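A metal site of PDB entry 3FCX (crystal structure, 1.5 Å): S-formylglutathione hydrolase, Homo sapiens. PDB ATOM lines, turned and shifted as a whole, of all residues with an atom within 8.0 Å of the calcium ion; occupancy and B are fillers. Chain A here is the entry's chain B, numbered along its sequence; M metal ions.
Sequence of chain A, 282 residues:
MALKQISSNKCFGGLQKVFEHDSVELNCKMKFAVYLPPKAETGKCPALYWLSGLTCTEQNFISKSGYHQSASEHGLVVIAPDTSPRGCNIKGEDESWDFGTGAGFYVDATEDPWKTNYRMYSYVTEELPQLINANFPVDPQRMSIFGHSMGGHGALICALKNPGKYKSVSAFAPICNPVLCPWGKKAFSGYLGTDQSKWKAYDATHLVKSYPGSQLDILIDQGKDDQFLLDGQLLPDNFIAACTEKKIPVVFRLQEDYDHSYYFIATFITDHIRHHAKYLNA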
ATOM      1  N   PRO A  37      -9.218  -3.644  12.265  1.00  0.00           N
ATOM      2  CA  PRO A  37      -8.457  -2.493  11.768  1.00  0.00           C
ATOM      3  C   PRO A  37      -7.669  -1.862  12.908  1.00  0.00           C
ATOM      4  O   PRO A  37      -7.924  -2.180  14.068  1.00  0.00           O
ATOM      5  CB  PRO A  37      -9.563  -1.546  11.282  1.00  0.00           C
ATOM      6  CG  PRO A  37     -10.733  -1.867  12.143  1.00  0.00           C
ATOM      7  CD  PRO A  37     -10.661  -3.368  12.271  1.00  0.00           C
ATOM      8  N   LYS A  39      -8.034   0.780  14.302  1.00  0.00           N
ATOM      9  CA  LYS A  39      -9.035   1.324  15.227  1.00  0.00           C
ATOM     10  C   LYS A  39      -9.532   0.313  16.287  1.00  0.00           C
ATOM     11  O   LYS A  39      -9.797   0.661  17.421  1.00  0.00           O
ATOM     12  CB  LYS A  39     -10.252   1.843  14.466  1.00  0.00           C
ATOM     13  CG  LYS A  39     -11.091   2.809  15.276  1.00  0.00           C
ATOM     14  CD  LYS A  39     -12.171   3.563  14.447  1.00  0.00           C
ATOM     15  CE  LYS A  39     -13.052   4.426  15.354  1.00  0.00           C
ATOM     16  NZ  LYS A  39     -14.250   4.847  14.673  1.00  0.00           N
ATOM     17  N   ALA A  40      -9.609  -0.945  15.881  1.00  0.00           N
ATOM     18  CA  ALA A  40     -10.104  -1.996  16.755  1.00  0.00           C
ATOM     19  C   ALA A  40      -9.133  -2.364  17.884  1.00  0.00           C
ATOM     20  O   ALA A  40      -8.867  -3.504  18.093  1.00  0.00           O
ATOM     21  CB  ALA A  40     -10.456  -3.287  15.918  1.00  0.00           C
ATOM     22  N   CYS A  45     -15.602  -0.719  17.024  1.00  0.00           N
ATOM     23  CA  CYS A  45     -15.785  -0.390  15.611  1.00  0.00           C
ATOM     24  C   CYS A  45     -17.122  -0.908  15.090  1.00  0.00           C
ATOM     25  O   CYS A  45     -17.649  -1.900  15.597  1.00  0.00           O
ATOM     26  CB  CYS A  45     -14.665  -1.008  14.764  1.00  0.00           C
ATOM     27  SG  CYS A  45     -12.998  -0.380  15.042  1.00  0.00           S
ATOM     28  N   PRO A  46     -17.678  -0.224  14.069  1.00  0.00           N
ATOM     29  CA  PRO A  46     -18.779  -0.840  13.329  1.00  0.00           C
ATOM     30  C   PRO A  46     -18.298  -2.104  12.628  1.00  0.00           C
ATOM     31  O   PRO A  46     -17.104  -2.246  12.332  1.00  0.00           O
ATOM     32  CB  PRO A  46     -19.146   0.216  12.289  1.00  0.00           C
ATOM     33  CG  PRO A  46     -18.616   1.488  12.811  1.00  0.00           C
ATOM     34  CD  PRO A  46     -17.385   1.130  13.581  1.00  0.00           C
ATOM     35  N   ALA A  47     -19.235  -3.006  12.358  1.00  0.00           N
ATOM     36  CA  ALA A  47     -18.937  -4.284  11.717  1.00  0.00           C
ATOM     37  C   ALA A  47     -19.538  -4.366  10.326  1.00  0.00           C
ATOM     38  O   ALA A  47     -20.653  -3.900  10.088  1.00  0.00           O
ATOM     39  CB  ALA A  47     -19.428  -5.433  12.570  1.00  0.00           C
ATOM     40  N   ALA A  71     -10.921  -0.890   4.353  1.00  0.00           N
ATOM     41  CA  ALA A  71     -11.452  -1.276   5.662  1.00  0.00           C
ATOM     42  C   ALA A  71     -10.603  -0.672   6.792  1.00  0.00           C
ATOM     43  O   ALA A  71     -11.146  -0.210   7.802  1.00  0.00           O
ATOM     44  CB  ALA A  71     -11.531  -2.794   5.801  1.00  0.00           C
ATOM     45  N   SER A  72      -9.290  -0.691   6.606  1.00  0.00           N
ATOM     46  CA  SER A  72      -8.351  -0.084   7.559  1.00  0.00           C
ATOM     47  C   SER A  72      -8.568   1.433   7.687  1.00  0.00           C
ATOM     48  O   SER A  72      -8.717   1.951   8.795  1.00  0.00           O
ATOM     49  CB  SER A  72      -6.914  -0.385   7.137  1.00  0.00           C
ATOM     50  OG  SER A  72      -5.981   0.219   8.019  1.00  0.00           O
ATOM     51  N   GLU A  73      -8.597   2.121   6.543  1.00  0.00           N
ATOM     52  CA  GLU A  73      -8.714   3.587   6.539  1.00  0.00           C
ATOM     53  C   GLU A  73     -10.055   4.067   7.107  1.00  0.00           C
ATOM     54  O   GLU A  73     -10.133   5.158   7.688  1.00  0.00           O
ATOM     55  CB  GLU A  73      -8.493   4.134   5.121  1.00  0.00           C
ATOM     56  CG  GLU A  73      -7.047   3.972   4.624  1.00  0.00           C
ATOM     57  CD  GLU A  73      -6.848   4.351   3.165  1.00  0.00           C
ATOM     58  OE1 GLU A  73      -7.849   4.612   2.457  1.00  0.00           O
ATOM     59  OE2 GLU A  73      -5.682   4.394   2.727  1.00  0.00           O
ATOM     60  N   HIS A  74     -11.092   3.257   6.963  1.00  0.00           N
ATOM     61  CA  HIS A  74     -12.415   3.613   7.467  1.00  0.00           C
ATOM     62  C   HIS A  74     -12.760   2.989   8.820  1.00  0.00           C
ATOM     63  O   HIS A  74     -13.869   3.190   9.349  1.00  0.00           O
ATOM     64  CB  HIS A  74     -13.489   3.304   6.420  1.00  0.00           C
ATOM     65  CG  HIS A  74     -13.412   4.212   5.235  1.00  0.00           C
ATOM     66  ND1 HIS A  74     -13.925   5.490   5.240  1.00  0.00           N
ATOM     67  CD2 HIS A  74     -12.857   4.036   4.005  1.00  0.00           C
ATOM     68  CE1 HIS A  74     -13.698   6.059   4.076  1.00  0.00           C
ATOM     69  NE2 HIS A  74     -13.056   5.202   3.309  1.00  0.00           N
ATOM     70  N   GLY A  75     -11.806   2.248   9.392  1.00  0.00           N
ATOM     71  CA  GLY A  75     -11.952   1.684  10.722  1.00  0.00           C
ATOM     72  C   GLY A  75     -13.121   0.727  10.867  1.00  0.00           C
ATOM     73  O   GLY A  75     -13.899   0.814  11.813  1.00  0.00           O
ATOM     74  N   LEU A  76     -13.238  -0.190   9.912  1.00  0.00           N
ATOM     75  CA  LEU A  76     -14.320  -1.171   9.937  1.00  0.00           C
ATOM     76  C   LEU A  76     -13.782  -2.545  10.265  1.00  0.00           C
ATOM     77  O   LEU A  76     -12.802  -2.995   9.662  1.00  0.00           O
ATOM     78  CB  LEU A  76     -15.065  -1.214   8.594  1.00  0.00           C
ATOM     79  CG  LEU A  76     -15.647   0.085   8.023  1.00  0.00           C
ATOM     80  CD1 LEU A  76     -16.335  -0.209   6.695  1.00  0.00           C
ATOM     81  CD2 LEU A  76     -16.615   0.756   8.995  1.00  0.00           C
ATOM     82  N   VAL A  77     -14.407  -3.201  11.248  1.00  0.00           N
ATOM     83  CA  VAL A  77     -14.182  -4.635  11.462  1.00  0.00           C
ATOM     84  C   VAL A  77     -14.948  -5.371  10.373  1.00  0.00           C
ATOM     85  O   VAL A  77     -16.116  -5.098  10.131  1.00  0.00           O
ATOM     86  CB  VAL A  77     -14.686  -5.079  12.857  1.00  0.00           C
ATOM     87  CG1 VAL A  77     -14.693  -6.603  12.979  1.00  0.00           C
ATOM     88  CG2 VAL A  77     -13.825  -4.471  13.958  1.00  0.00           C
ATOM     89  N   ARG A 142     -24.168  -1.075  15.218  1.00  0.00           N
ATOM     90  CA  ARG A 142     -23.729  -0.602  13.903  1.00  0.00           C
ATOM     91  C   ARG A 142     -23.125  -1.737  13.082  1.00  0.00           C
ATOM     92  O   ARG A 142     -21.960  -2.103  13.253  1.00  0.00           O
ATOM     93  CB  ARG A 142     -22.753   0.569  14.034  1.00  0.00           C
ATOM     94  CG  ARG A 142     -23.376   1.855  14.578  1.00  0.00           C
ATOM     95  CD  ARG A 142     -22.390   3.005  14.537  1.00  0.00           C
ATOM     96  NE  ARG A 142     -21.261   2.798  15.449  1.00  0.00           N
ATOM     97  CZ  ARG A 142     -20.121   3.488  15.434  1.00  0.00           C
ATOM     98  NH1 ARG A 142     -19.922   4.449  14.544  1.00  0.00           N
ATOM     99  NH2 ARG A 142     -19.178   3.196  16.317  1.00  0.00           N
ATOM    100  N   ALA A 277     -19.061   2.624   4.864  1.00  0.00           N
ATOM    101  CA  ALA A 277     -18.485   3.566   5.836  1.00  0.00           C
ATOM    102  C   ALA A 277     -19.356   4.803   5.999  1.00  0.00           C
ATOM    103  O   ALA A 277     -19.486   5.320   7.118  1.00  0.00           O
ATOM    104  CB  ALA A 277     -17.072   3.947   5.438  1.00  0.00           C
ATOM    105  N   LEU A 280     -22.090   3.558   8.307  1.00  0.00           N
ATOM    106  CA  LEU A 280     -21.620   2.985   9.567  1.00  0.00           C
ATOM    107  C   LEU A 280     -20.922   4.012  10.463  1.00  0.00           C
ATOM    108  O   LEU A 280     -21.049   3.963  11.691  1.00  0.00           O
ATOM    109  CB  LEU A 280     -20.686   1.801   9.312  1.00  0.00           C
ATOM    110  CG  LEU A 280     -21.315   0.507   8.772  1.00  0.00           C
ATOM    111  CD1 LEU A 280     -20.234  -0.422   8.262  1.00  0.00           C
ATOM    112  CD2 LEU A 280     -22.173  -0.186   9.829  1.00  0.00           C
ATOM    113  N   ASN A 281     -20.197   4.933   9.848  1.00  0.00           N
ATOM    114  CA  ASN A 281     -19.490   5.989  10.567  1.00  0.00           C
ATOM    115  C   ASN A 281     -20.265   7.307  10.573  1.00  0.00           C
ATOM    116  O   ASN A 281     -20.050   8.157  11.435  1.00  0.00           O
ATOM    117  CB  ASN A 281     -18.082   6.208   9.990  1.00  0.00           C
ATOM    118  CG  ASN A 281     -17.190   4.985  10.162  1.00  0.00           C
ATOM    119  OD1 ASN A 281     -17.300   4.240  11.131  1.00  0.00           O
ATOM    120  ND2 ASN A 281     -16.278   4.792   9.211  1.00  0.00           N
HETATM  121 CA    CA M   1     -14.987   3.386  12.396  1.00  0.00          CA
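O of Gly 75 sits close to SG of Cys 45, at 3.6 Å.
N of Val 77 is in hydrogen-bond range of O of Pro 46 (3.1 Å).
The side-chain amide nitrogen of Asn 281 sits at hydrogen-bond distance from the backbone carbonyl oxygen of His 74 (2.9 Å).
Residues that only touch the calcium ion: Pro 46 (3.5 Å) and His 74 (3.3 Å).
Within 4 Å of the calcium ion: Lys 39, Pro 46, His 74, Gly 75 and Asn 281.
OD1 of Asn 281 is bound to the calcium ion, 2.8 Å away.
The calcium ion is bound by NZ of Lys 39 (2.8 Å).
The backbone carbonyl oxygen (O) of Gly 75 binds the calcium ion (2.9 Å).
The calcium ion has three donor atoms within binding distance.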
